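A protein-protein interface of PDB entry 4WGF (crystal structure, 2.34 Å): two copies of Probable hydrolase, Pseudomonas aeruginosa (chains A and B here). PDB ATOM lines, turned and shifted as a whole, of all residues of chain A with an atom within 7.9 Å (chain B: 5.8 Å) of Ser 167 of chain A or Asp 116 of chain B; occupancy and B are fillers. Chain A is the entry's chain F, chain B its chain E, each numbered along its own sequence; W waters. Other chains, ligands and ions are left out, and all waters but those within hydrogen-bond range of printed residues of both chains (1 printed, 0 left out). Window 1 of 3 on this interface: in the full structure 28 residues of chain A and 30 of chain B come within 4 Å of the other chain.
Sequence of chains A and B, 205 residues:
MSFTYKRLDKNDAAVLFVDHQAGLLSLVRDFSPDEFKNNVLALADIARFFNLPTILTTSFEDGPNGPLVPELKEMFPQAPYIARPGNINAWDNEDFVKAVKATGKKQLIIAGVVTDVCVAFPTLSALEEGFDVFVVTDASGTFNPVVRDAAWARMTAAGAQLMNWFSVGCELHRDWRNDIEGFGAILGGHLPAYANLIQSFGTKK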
ATOM      1  N   TYR A   5      22.391 -18.537  -0.828  1.00  0.00           N
ATOM      2  CA  TYR A   5      21.481 -19.440  -1.516  1.00  0.00           C
ATOM      3  C   TYR A   5      20.908 -18.779  -2.768  1.00  0.00           C
ATOM      4  O   TYR A   5      19.861 -18.137  -2.708  1.00  0.00           O
ATOM      5  CB  TYR A   5      20.357 -19.865  -0.561  1.00  0.00           C
ATOM      6  CG  TYR A   5      19.369 -20.886  -1.095  1.00  0.00           C
ATOM      7  CD1 TYR A   5      19.623 -21.603  -2.258  1.00  0.00           C
ATOM      8  CD2 TYR A   5      18.179 -21.132  -0.424  1.00  0.00           C
ATOM      9  CE1 TYR A   5      18.715 -22.530  -2.738  1.00  0.00           C
ATOM     10  CE2 TYR A   5      17.267 -22.059  -0.894  1.00  0.00           C
ATOM     11  CZ  TYR A   5      17.540 -22.756  -2.050  1.00  0.00           C
ATOM     12  OH  TYR A   5      16.632 -23.678  -2.518  1.00  0.00           O
ATOM     13  N   LEU A   8      16.426 -20.407  -7.864  1.00  0.00           N
ATOM     14  CA  LEU A   8      15.733 -19.984  -9.073  1.00  0.00           C
ATOM     15  C   LEU A   8      14.598 -19.008  -8.791  1.00  0.00           C
ATOM     16  O   LEU A   8      13.788 -19.216  -7.889  1.00  0.00           O
ATOM     17  CB  LEU A   8      15.192 -21.204  -9.820  1.00  0.00           C
ATOM     18  CG  LEU A   8      16.236 -22.019 -10.583  1.00  0.00           C
ATOM     19  CD1 LEU A   8      15.647 -23.329 -11.079  1.00  0.00           C
ATOM     20  CD2 LEU A   8      16.785 -21.202 -11.741  1.00  0.00           C
ATOM     21  N   ILE A  46       7.380 -27.066 -17.636  1.00  0.00           N
ATOM     22  CA  ILE A  46       7.726 -26.140 -16.563  1.00  0.00           C
ATOM     23  C   ILE A  46       8.077 -24.771 -17.133  1.00  0.00           C
ATOM     24  O   ILE A  46       7.639 -23.740 -16.618  1.00  0.00           O
ATOM     25  CB  ILE A  46       8.901 -26.677 -15.723  1.00  0.00           C
ATOM     26  CG1 ILE A  46       8.446 -27.874 -14.890  1.00  0.00           C
ATOM     27  CG2 ILE A  46       9.468 -25.590 -14.821  1.00  0.00           C
ATOM     28  CD1 ILE A  46       9.563 -28.550 -14.143  1.00  0.00           C
ATOM     29  N   VAL A 135      21.946 -26.425 -14.109  1.00  0.00           N
ATOM     30  CA  VAL A 135      21.952 -27.532 -15.058  1.00  0.00           C
ATOM     31  C   VAL A 135      20.915 -28.590 -14.695  1.00  0.00           C
ATOM     32  O   VAL A 135      20.925 -29.127 -13.587  1.00  0.00           O
ATOM     33  CB  VAL A 135      23.345 -28.193 -15.143  1.00  0.00           C
ATOM     34  CG1 VAL A 135      23.335 -29.326 -16.155  1.00  0.00           C
ATOM     35  CG2 VAL A 135      24.400 -27.161 -15.509  1.00  0.00           C
ATOM     36  N   VAL A 136      20.019 -28.884 -15.633  1.00  0.00           N
ATOM     37  CA  VAL A 136      19.038 -29.944 -15.446  1.00  0.00           C
ATOM     38  C   VAL A 136      19.649 -31.283 -15.840  1.00  0.00           C
ATOM     39  O   VAL A 136      19.623 -31.674 -17.008  1.00  0.00           O
ATOM     40  CB  VAL A 136      17.762 -29.700 -16.266  1.00  0.00           C
ATOM     41  CG1 VAL A 136      16.649 -30.613 -15.783  1.00  0.00           C
ATOM     42  CG2 VAL A 136      17.337 -28.241 -16.166  1.00  0.00           C
ATOM     43  N   THR A 137      20.202 -31.976 -14.852  1.00  0.00           N
ATOM     44  CA  THR A 137      21.022 -33.157 -15.095  1.00  0.00           C
ATOM     45  C   THR A 137      20.260 -34.342 -15.685  1.00  0.00           C
ATOM     46  O   THR A 137      20.836 -35.147 -16.417  1.00  0.00           O
ATOM     47  CB  THR A 137      21.702 -33.621 -13.797  1.00  0.00           C
ATOM     48  OG1 THR A 137      20.704 -33.947 -12.821  1.00  0.00           O
ATOM     49  CG2 THR A 137      22.603 -32.526 -13.245  1.00  0.00           C
ATOM     50  N   ASP A 138      18.973 -34.458 -15.369  1.00  0.00           N
ATOM     51  CA  ASP A 138      18.198 -35.592 -15.861  1.00  0.00           C
ATOM     52  C   ASP A 138      17.480 -35.265 -17.168  1.00  0.00           C
ATOM     53  O   ASP A 138      16.809 -36.118 -17.745  1.00  0.00           O
ATOM     54  CB  ASP A 138      17.193 -36.060 -14.803  1.00  0.00           C
ATOM     55  CG  ASP A 138      16.245 -34.965 -14.364  1.00  0.00           C
ATOM     56  OD1 ASP A 138      16.470 -33.791 -14.727  1.00  0.00           O
ATOM     57  OD2 ASP A 138      15.268 -35.283 -13.653  1.00  0.00           O
ATOM     58  N   LEU A 162      24.019 -28.026  -9.992  1.00  0.00           N
ATOM     59  CA  LEU A 162      23.440 -29.240 -10.554  1.00  0.00           C
ATOM     60  C   LEU A 162      22.073 -29.518  -9.947  1.00  0.00           C
ATOM     61  O   LEU A 162      21.930 -29.595  -8.727  1.00  0.00           O
ATOM     62  CB  LEU A 162      24.368 -30.434 -10.326  1.00  0.00           C
ATOM     63  CG  LEU A 162      25.786 -30.312 -10.882  1.00  0.00           C
ATOM     64  CD1 LEU A 162      26.553 -31.608 -10.674  1.00  0.00           C
ATOM     65  CD2 LEU A 162      25.755 -29.926 -12.355  1.00  0.00           C
ATOM     66  N   MET A 163      21.068 -29.660 -10.807  1.00  0.00           N
ATOM     67  CA  MET A 163      19.708 -29.925 -10.358  1.00  0.00           C
ATOM     68  C   MET A 163      18.997 -30.907 -11.285  1.00  0.00           C
ATOM     69  O   MET A 163      19.628 -31.594 -12.088  1.00  0.00           O
ATOM     70  CB  MET A 163      18.907 -28.620 -10.265  1.00  0.00           C
ATOM     71  CG  MET A 163      19.459 -27.622  -9.253  1.00  0.00           C
ATOM     72  SD  MET A 163      18.478 -25.941  -9.152  1.00  0.00           S
ATOM     73  CE  MET A 163      16.810 -26.605  -8.394  1.00  0.00           C
ATOM     74  N   ASN A 164      17.677 -30.963 -11.155  1.00  0.00           N
ATOM     75  CA  ASN A 164      16.829 -31.811 -11.983  1.00  0.00           C
ATOM     76  C   ASN A 164      15.512 -31.092 -12.230  1.00  0.00           C
ATOM     77  O   ASN A 164      15.225 -30.099 -11.562  1.00  0.00           O
ATOM     78  CB  ASN A 164      16.596 -33.166 -11.316  1.00  0.00           C
ATOM     79  CG  ASN A 164      16.174 -33.034  -9.865  1.00  0.00           C
ATOM     80  OD1 ASN A 164      16.965 -32.633  -9.011  1.00  0.00           O
ATOM     81  ND2 ASN A 164      14.922 -33.373  -9.579  1.00  0.00           N
ATOM     82  N   TRP A 165      14.716 -31.575 -13.180  1.00  0.00           N
ATOM     83  CA  TRP A 165      13.521 -30.842 -13.589  1.00  0.00           C
ATOM     84  C   TRP A 165      12.543 -30.661 -12.433  1.00  0.00           C
ATOM     85  O   TRP A 165      11.895 -29.621 -12.327  1.00  0.00           O
ATOM     86  CB  TRP A 165      12.827 -31.525 -14.776  1.00  0.00           C
ATOM     87  CG  TRP A 165      12.168 -32.846 -14.486  1.00  0.00           C
ATOM     88  CD1 TRP A 165      12.679 -34.086 -14.737  1.00  0.00           C
ATOM     89  CD2 TRP A 165      10.865 -33.057 -13.920  1.00  0.00           C
ATOM     90  NE1 TRP A 165      11.783 -35.055 -14.354  1.00  0.00           N
ATOM     91  CE2 TRP A 165      10.662 -34.450 -13.849  1.00  0.00           C
ATOM     92  CE3 TRP A 165       9.854 -32.204 -13.465  1.00  0.00           C
ATOM     93  CZ2 TRP A 165       9.492 -35.008 -13.338  1.00  0.00           C
ATOM     94  CZ3 TRP A 165       8.695 -32.761 -12.956  1.00  0.00           C
ATOM     95  CH2 TRP A 165       8.523 -34.151 -12.898  1.00  0.00           C
ATOM     96  N   PHE A 166      12.444 -31.659 -11.561  1.00  0.00           N
ATOM     97  CA  PHE A 166      11.524 -31.572 -10.432  1.00  0.00           C
ATOM     98  C   PHE A 166      11.962 -30.505  -9.432  1.00  0.00           C
ATOM     99  O   PHE A 166      11.139 -29.725  -8.951  1.00  0.00           O
ATOM    100  CB  PHE A 166      11.387 -32.921  -9.726  1.00  0.00           C
ATOM    101  CG  PHE A 166      10.424 -32.900  -8.573  1.00  0.00           C
ATOM    102  CD1 PHE A 166       9.058 -32.948  -8.795  1.00  0.00           C
ATOM    103  CD2 PHE A 166      10.883 -32.828  -7.268  1.00  0.00           C
ATOM    104  CE1 PHE A 166       8.167 -32.923  -7.738  1.00  0.00           C
ATOM    105  CE2 PHE A 166       9.997 -32.805  -6.207  1.00  0.00           C
ATOM    106  CZ  PHE A 166       8.637 -32.853  -6.443  1.00  0.00           C
ATOM    107  N   SER A 167      13.252 -30.474  -9.116  1.00  0.00           N
ATOM    108  CA  SER A 167      13.770 -29.486  -8.179  1.00  0.00           C
ATOM    109  C   SER A 167      13.707 -28.093  -8.797  1.00  0.00           C
ATOM    110  O   SER A 167      13.471 -27.108  -8.098  1.00  0.00           O
ATOM    111  CB  SER A 167      15.202 -29.826  -7.758  1.00  0.00           C
ATOM    112  OG  SER A 167      16.071 -29.875  -8.875  1.00  0.00           O
ATOM    113  N   VAL A 168      13.923 -28.020 -10.107  1.00  0.00           N
ATOM    114  CA  VAL A 168      13.787 -26.764 -10.839  1.00  0.00           C
ATOM    115  C   VAL A 168      12.356 -26.245 -10.723  1.00  0.00           C
ATOM    116  O   VAL A 168      12.132 -25.067 -10.443  1.00  0.00           O
ATOM    117  CB  VAL A 168      14.164 -26.924 -12.328  1.00  0.00           C
ATOM    118  CG1 VAL A 168      13.651 -25.747 -13.143  1.00  0.00           C
ATOM    119  CG2 VAL A 168      15.669 -27.067 -12.487  1.00  0.00           C
ATOM    120  N   GLY A 169      11.394 -27.140 -10.928  1.00  0.00           N
ATOM    121  CA  GLY A 169       9.988 -26.791 -10.833  1.00  0.00           C
ATOM    122  C   GLY A 169       9.583 -26.324  -9.447  1.00  0.00           C
ATOM    123  O   GLY A 169       8.857 -25.341  -9.307  1.00  0.00           O
ATOM    124  N   CYS A 170      10.053 -27.027  -8.420  1.00  0.00           N
ATOM    125  CA  CYS A 170       9.708 -26.690  -7.041  1.00  0.00           C
ATOM    126  C   CYS A 170      10.356 -25.387  -6.580  1.00  0.00           C
ATOM    127  O   CYS A 170       9.761 -24.626  -5.818  1.00  0.00           O
ATOM    128  CB  CYS A 170      10.111 -27.826  -6.099  1.00  0.00           C
ATOM    129  SG  CYS A 170       9.113 -29.322  -6.262  1.00  0.00           S
ATOM    130  N   GLU A 171      11.576 -25.133  -7.042  1.00  0.00           N
ATOM    131  CA  GLU A 171      12.291 -23.923  -6.659  1.00  0.00           C
ATOM    132  C   GLU A 171      11.699 -22.699  -7.349  1.00  0.00           C
ATOM    133  O   GLU A 171      11.740 -21.592  -6.814  1.00  0.00           O
ATOM    134  CB  GLU A 171      13.781 -24.055  -6.979  1.00  0.00           C
ATOM    135  CG  GLU A 171      14.649 -22.998  -6.316  1.00  0.00           C
ATOM    136  CD  GLU A 171      16.098 -23.426  -6.192  1.00  0.00           C
ATOM    137  OE1 GLU A 171      16.427 -24.147  -5.226  1.00  0.00           O
ATOM    138  OE2 GLU A 171      16.911 -23.037  -7.057  1.00  0.00           O
ATOM    139  N   LEU A 172      11.153 -22.902  -8.543  1.00  0.00           N
ATOM    140  CA  LEU A 172      10.478 -21.827  -9.260  1.00  0.00           C
ATOM    141  C   LEU A 172       9.104 -21.545  -8.655  1.00  0.00           C
ATOM    142  O   LEU A 172       8.687 -20.391  -8.553  1.00  0.00           O
ATOM    143  CB  LEU A 172      10.339 -22.172 -10.745  1.00  0.00           C
ATOM    144  CG  LEU A 172      11.605 -22.082 -11.599  1.00  0.00           C
ATOM    145  CD1 LEU A 172      11.388 -22.740 -12.953  1.00  0.00           C
ATOM    146  CD2 LEU A 172      12.040 -20.633 -11.765  1.00  0.00           C
ATOM    147  N   HIS A 173       8.408 -22.604  -8.250  1.00  0.00           N
ATOM    148  CA  HIS A 173       7.033 -22.488  -7.772  1.00  0.00           C
ATOM    149  C   HIS A 173       6.939 -21.941  -6.348  1.00  0.00           C
ATOM    150  O   HIS A 173       5.998 -21.213  -6.024  1.00  0.00           O
ATOM    151  CB  HIS A 173       6.333 -23.847  -7.852  1.00  0.00           C
ATOM    152  CG  HIS A 173       4.845 -23.767  -7.736  1.00  0.00           C
ATOM    153  ND1 HIS A 173       4.085 -22.876  -8.467  1.00  0.00           N
ATOM    154  CD2 HIS A 173       3.969 -24.467  -6.977  1.00  0.00           C
ATOM    155  CE1 HIS A 173       2.811 -23.031  -8.162  1.00  0.00           C
ATOM    156  NE2 HIS A 173       2.713 -23.992  -7.259  1.00  0.00           N
ATOM    157  N   ARG A 174       7.901 -22.314  -5.503  1.00  0.00           N
ATOM    158  CA  ARG A 174       7.989 -21.837  -4.118  1.00  0.00           C
ATOM    159  C   ARG A 174       6.815 -22.268  -3.240  1.00  0.00           C
ATOM    160  O   ARG A 174       7.004 -22.907  -2.205  1.00  0.00           O
ATOM    161  CB  ARG A 174       8.103 -20.310  -4.082  1.00  0.00           C
ATOM    162  CG  ARG A 174       9.273 -19.744  -4.860  1.00  0.00           C
ATOM    163  CD  ARG A 174      10.597 -20.131  -4.234  1.00  0.00           C
ATOM    164  NE  ARG A 174      11.717 -19.523  -4.945  1.00  0.00           N
ATOM    165  CZ  ARG A 174      12.201 -18.315  -4.678  1.00  0.00           C
ATOM    166  NH1 ARG A 174      11.664 -17.581  -3.713  1.00  0.00           N
ATOM    167  NH2 ARG A 174      13.222 -17.839  -5.378  1.00  0.00           N
ATOM    168  N   PHE A 183       0.099 -26.636 -11.136  1.00  0.00           N
ATOM    169  CA  PHE A 183       1.383 -27.230 -10.792  1.00  0.00           C
ATOM    170  C   PHE A 183       1.234 -28.735 -10.589  1.00  0.00           C
ATOM    171  O   PHE A 183       2.121 -29.509 -10.948  1.00  0.00           O
ATOM    172  CB  PHE A 183       1.962 -26.582  -9.535  1.00  0.00           C
ATOM    173  CG  PHE A 183       3.370 -27.002  -9.235  1.00  0.00           C
ATOM    174  CD1 PHE A 183       4.411 -26.610 -10.061  1.00  0.00           C
ATOM    175  CD2 PHE A 183       3.654 -27.788  -8.132  1.00  0.00           C
ATOM    176  CE1 PHE A 183       5.710 -26.995  -9.792  1.00  0.00           C
ATOM    177  CE2 PHE A 183       4.952 -28.176  -7.856  1.00  0.00           C
ATOM    178  CZ  PHE A 183       5.981 -27.779  -8.688  1.00  0.00           C
ATOM    179  N   VAL B 114      11.397 -35.139  -0.814  1.00  0.00           N
ATOM    180  CA  VAL B 114      12.534 -35.801  -1.443  1.00  0.00           C
ATOM    181  C   VAL B 114      13.839 -35.053  -1.169  1.00  0.00           C
ATOM    182  O   VAL B 114      13.825 -33.887  -0.775  1.00  0.00           O
ATOM    183  CB  VAL B 114      12.341 -35.928  -2.971  1.00  0.00           C
ATOM    184  CG1 VAL B 114      11.240 -36.928  -3.297  1.00  0.00           C
ATOM    185  CG2 VAL B 114      12.035 -34.571  -3.582  1.00  0.00           C
ATOM    186  N   THR B 115      14.961 -35.735  -1.382  1.00  0.00           N
ATOM    187  CA  THR B 115      16.279 -35.196  -1.058  1.00  0.00           C
ATOM    188  C   THR B 115      16.603 -33.905  -1.809  1.00  0.00           C
ATOM    189  O   THR B 115      17.082 -32.935  -1.221  1.00  0.00           O
ATOM    190  CB  THR B 115      17.389 -36.221  -1.368  1.00  0.00           C
ATOM    191  OG1 THR B 115      17.058 -37.485  -0.779  1.00  0.00           O
ATOM    192  CG2 THR B 115      18.728 -35.740  -0.826  1.00  0.00           C
ATOM    193  N   ASP B 116      16.332 -33.898  -3.110  1.00  0.00           N
ATOM    194  CA  ASP B 116      16.707 -32.783  -3.973  1.00  0.00           C
ATOM    195  C   ASP B 116      15.876 -31.523  -3.747  1.00  0.00           C
ATOM    196  O   ASP B 116      16.217 -30.452  -4.252  1.00  0.00           O
ATOM    197  CB  ASP B 116      16.601 -33.203  -5.438  1.00  0.00           C
ATOM    198  CG  ASP B 116      15.282 -33.878  -5.751  1.00  0.00           C
ATOM    199  OD1 ASP B 116      14.919 -34.833  -5.033  1.00  0.00           O
ATOM    200  OD2 ASP B 116      14.608 -33.458  -6.716  1.00  0.00           O
ATOM    201  N   VAL B 117      14.788 -31.645  -2.995  1.00  0.00           N
ATOM    202  CA  VAL B 117      13.892 -30.514  -2.787  1.00  0.00           C
ATOM    203  C   VAL B 117      13.621 -30.250  -1.310  1.00  0.00           C
ATOM    204  O   VAL B 117      14.074 -29.248  -0.758  1.00  0.00           O
ATOM    205  CB  VAL B 117      12.546 -30.725  -3.506  1.00  0.00           C
ATOM    206  CG1 VAL B 117      11.591 -29.591  -3.187  1.00  0.00           C
ATOM    207  CG2 VAL B 117      12.759 -30.826  -5.002  1.00  0.00           C
ATOM    208  N   CYS B 118      12.883 -31.153  -0.673  1.00  0.00           N
ATOM    209  CA  CYS B 118      12.420 -30.933   0.693  1.00  0.00           C
ATOM    210  C   CYS B 118      13.552 -31.040   1.709  1.00  0.00           C
ATOM    211  O   CYS B 118      13.405 -30.630   2.859  1.00  0.00           O
ATOM    212  CB  CYS B 118      11.303 -31.919   1.034  1.00  0.00           C
ATOM    213  SG  CYS B 118       9.899 -31.850  -0.109  1.00  0.00           S
ATOM    214  N   VAL B 119      14.681 -31.596   1.283  1.00  0.00           N
ATOM    215  CA  VAL B 119      15.872 -31.641   2.121  1.00  0.00           C
ATOM    216  C   VAL B 119      16.863 -30.564   1.700  1.00  0.00           C
ATOM    217  O   VAL B 119      17.367 -29.807   2.529  1.00  0.00           O
ATOM    218  CB  VAL B 119      16.567 -33.012   2.054  1.00  0.00           C
ATOM    219  CG1 VAL B 119      17.887 -32.975   2.811  1.00  0.00           C
ATOM    220  CG2 VAL B 119      15.662 -34.090   2.612  1.00  0.00           C
ATOM    221  N   ALA B 120      17.132 -30.506   0.399  1.00  0.00           N
ATOM    222  CA  ALA B 120      18.129 -29.597  -0.152  1.00  0.00           C
ATOM    223  C   ALA B 120      17.792 -28.132   0.104  1.00  0.00           C
ATOM    224  O   ALA B 120      18.647 -27.367   0.541  1.00  0.00           O
ATOM    225  CB  ALA B 120      18.292 -29.843  -1.644  1.00  0.00           C
ATOM    226  N   PHE B 121      16.545 -27.749  -0.156  1.00  0.00           N
ATOM    227  CA  PHE B 121      16.149 -26.343  -0.067  1.00  0.00           C
ATOM    228  C   PHE B 121      16.303 -25.770   1.349  1.00  0.00           C
ATOM    229  O   PHE B 121      16.909 -24.710   1.509  1.00  0.00           O
ATOM    230  CB  PHE B 121      14.705 -26.141  -0.557  1.00  0.00           C
ATOM    231  CG  PHE B 121      14.508 -26.387  -2.032  1.00  0.00           C
ATOM    232  CD1 PHE B 121      15.566 -26.762  -2.847  1.00  0.00           C
ATOM    233  CD2 PHE B 121      13.256 -26.229  -2.605  1.00  0.00           C
ATOM    234  CE1 PHE B 121      15.375 -26.985  -4.199  1.00  0.00           C
ATOM    235  CE2 PHE B 121      13.060 -26.447  -3.956  1.00  0.00           C
ATOM    236  CZ  PHE B 121      14.120 -26.827  -4.754  1.00  0.00           C
ATOM    237  N   GLY B 141      15.306 -39.765   0.826  1.00  0.00           N
ATOM    238  CA  GLY B 141      15.065 -40.492  -0.406  1.00  0.00           C
ATOM    239  C   GLY B 141      14.641 -39.605  -1.556  1.00  0.00           C
ATOM    240  O   GLY B 141      14.143 -38.503  -1.348  1.00  0.00           O
ATOM    241  N   THR B 142      14.845 -40.090  -2.776  1.00  0.00           N
ATOM    242  CA  THR B 142      14.441 -39.357  -3.969  1.00  0.00           C
ATOM    243  C   THR B 142      14.182 -40.316  -5.132  1.00  0.00           C
ATOM    244  O   THR B 142      14.176 -41.534  -4.949  1.00  0.00           O
ATOM    245  CB  THR B 142      15.502 -38.311  -4.371  1.00  0.00           C
ATOM    246  OG1 THR B 142      15.007 -37.509  -5.451  1.00  0.00           O
ATOM    247  CG2 THR B 142      16.796 -38.988  -4.791  1.00  0.00           C
ATOM    248  N   PHE B 143      13.969 -39.761  -6.321  1.00  0.00           N
ATOM    249  CA  PHE B 143      13.498 -40.536  -7.470  1.00  0.00           C
ATOM    250  C   PHE B 143      14.474 -41.609  -7.951  1.00  0.00           C
ATOM    251  O   PHE B 143      14.054 -42.698  -8.343  1.00  0.00           O
ATOM    252  CB  PHE B 143      13.171 -39.593  -8.629  1.00  0.00           C
ATOM    253  CG  PHE B 143      12.276 -38.451  -8.244  1.00  0.00           C
ATOM    254  CD1 PHE B 143      10.911 -38.638  -8.111  1.00  0.00           C
ATOM    255  CD2 PHE B 143      12.801 -37.190  -8.014  1.00  0.00           C
ATOM    256  CE1 PHE B 143      10.084 -37.590  -7.757  1.00  0.00           C
ATOM    257  CE2 PHE B 143      11.979 -36.138  -7.660  1.00  0.00           C
ATOM    258  CZ  PHE B 143      10.619 -36.338  -7.531  1.00  0.00           C
ATOM    259  N   VAL B 147      19.495 -38.227  -9.432  1.00  0.00           N
ATOM    260  CA  VAL B 147      18.923 -37.054  -8.782  1.00  0.00           C
ATOM    261  C   VAL B 147      19.534 -36.870  -7.393  1.00  0.00           C
ATOM    262  O   VAL B 147      19.802 -35.747  -6.964  1.00  0.00           O
ATOM    263  CB  VAL B 147      17.386 -37.165  -8.673  1.00  0.00           C
ATOM    264  CG1 VAL B 147      16.822 -36.014  -7.868  1.00  0.00           C
ATOM    265  CG2 VAL B 147      16.756 -37.202 -10.058  1.00  0.00           C
ATOM    266  N   ALA B 151      21.860 -33.709  -5.911  1.00  0.00           N
ATOM    267  CA  ALA B 151      21.473 -33.030  -4.681  1.00  0.00           C
ATOM    268  C   ALA B 151      22.654 -32.952  -3.724  1.00  0.00           C
ATOM    269  O   ALA B 151      22.853 -31.940  -3.052  1.00  0.00           O
ATOM    270  CB  ALA B 151      20.303 -33.739  -4.026  1.00  0.00           C
ATOM    271  N   ARG B 154      25.098 -30.228  -4.879  1.00  0.00           N
ATOM    272  CA  ARG B 154      24.604 -28.888  -4.599  1.00  0.00           C
ATOM    273  C   ARG B 154      24.731 -28.548  -3.118  1.00  0.00           C
ATOM    274  O   ARG B 154      25.028 -27.409  -2.757  1.00  0.00           O
ATOM    275  CB  ARG B 154      23.149 -28.743  -5.044  1.00  0.00           C
ATOM    276  CG  ARG B 154      22.711 -27.298  -5.206  1.00  0.00           C
ATOM    277  CD  ARG B 154      21.231 -27.183  -5.517  1.00  0.00           C
ATOM    278  NE  ARG B 154      20.857 -25.806  -5.827  1.00  0.00           N
ATOM    279  CZ  ARG B 154      19.612 -25.342  -5.795  1.00  0.00           C
ATOM    280  NH1 ARG B 154      18.610 -26.142  -5.458  1.00  0.00           N
ATOM    281  NH2 ARG B 154      19.370 -24.072  -6.094  1.00  0.00           N
HETATM  282  O   HOH W   1      19.431 -32.809  -7.667  1.00  0.00           O
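No position is printed for both chains.
Among the printed residues, 17 pairs touch across the chains. Among the printed residues, Asp or Glu carboxylates within 4 Å of a Lys or Arg side-chain nitrogen of the other chain: Glu 171 of chain A with Arg 154 of chain B (2.8 Å).
ND2 of Asn 164 of chain A sits at hydrogen-bond distance from OD2 of Asp 116 of chain B, 2.9 Å away. The guanidinium group (NH2) of Arg 154 of chain B lies close to the side-chain sulfur (SD) of Met 163 of chain A (3.7 Å). OE2 of Glu 171 of chain A is in salt-bridge range of NH2 of Arg 154 of chain B.
Water W1 lies within hydrogen-bond range of OD1 of Asn 164 of chain A (2.8 Å), O of Val 147 of chain B (3.0 Å) and N of Ala 151 of chain B (3.1 Å).
Printed residues of chain B within 4 Å of Tyr 5 of chain A: Phe 121 and Arg 154. Printed residues of chain B within 4 Å of Asn 164 of chain A: Asp 116 (2.9 Å) and Val 147 (3.6 Å). Printed residues of chain B within 4 Å of Phe 166 of chain A: Val 114 (3.8 Å), Asp 116 (3.8 Å), Val 117 (3.6 Å) and Phe 143 (3.5 Å). Of chain B, only Asp 116 (3.7 Å), Val 117 (3.6 Å) and Phe 121 (3.4 Å) come within 4 Å of Ser 167 of chain A. Asp 116 of chain B touches just these residues of chain A: Asn 164 (2.9 Å), Phe 166 (3.8 Å) and Ser 167 (3.7 Å). Of the printed residues of chain A, Phe 121 of chain B touches Tyr 5 (3.3 Å), Ser 167 (3.4 Å), Cys 170 (3.9 Å) and Glu 171 (3.2 Å). Of the printed residues of chain A, Phe 143 of chain B touches Phe 166 (3.5 Å). The nearest residue of chain A that does not touch Asp 116 of chain B is Met 163 of chain A (5.7 Å). The nearest printed residue of chain B that does not touch Tyr 5 of chain A is Ala 120 of chain B (5.2 Å).
Among the printed residues, pairs that only touch across the chains: Tyr 5 of chain A with Phe 121 of chain B (3.3 Å), Tyr 5 of chain A with Arg 154 of chain B (3.8 Å), Leu 162 of chain A with Arg 154 of chain B (3.97 Å), Asn 164 of chain A with Val 147 of chain B (3.6 Å), Phe 166 of chain A with Val 114 of chain B (3.8 Å), Phe 166 of chain A with Asp 116 of chain B (3.8 Å), Phe 166 of chain A with Val 117 of chain B (3.6 Å), Phe 166 of chain A with Phe 143 of chain B (3.5 Å), Ser 167 of chain A with Asp 116 of chain B (3.7 Å), Ser 167 of chain A with Val 117 of chain B (3.6 Å), Ser 167 of chain A with Phe 121 of chain B (3.4 Å), Cys 170 of chain A with Val 117 of chain B (3.7 Å), Cys 170 of chain A with Phe 121 of chain B (3.9 Å) and Glu 171 of chain A with Phe 121 of chain B (3.2 Å).
SG of Cys 118 of chain B sits at hydrogen-bond distance from N of Val 114 of chain B. The backbone NH (N) of Val 119 of chain B is in hydrogen-bond range of the backbone carbonyl oxygen (O) of Val 114 of chain B, 3.2 Å away. The side-chain carboxylate of Asp 116 of chain B sits at hydrogen-bond distance from the side-chain hydroxyl of Thr 142 of chain B (2.7 Å). The backbone carbonyl oxygen (O) of Val 135 of chain A lies within hydrogen-bond range of the backbone NH (N) of Met 163 of chain A, at 2.8 Å. The backbone carbonyl oxygen of Met 163 of chain A is in hydrogen-bond range of the side-chain hydroxyl of Thr 137 of chain A (2.7 Å). OG of Ser 167 of chain A is in hydrogen-bond range of O of Asn 164 of chain A (2.8 Å).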
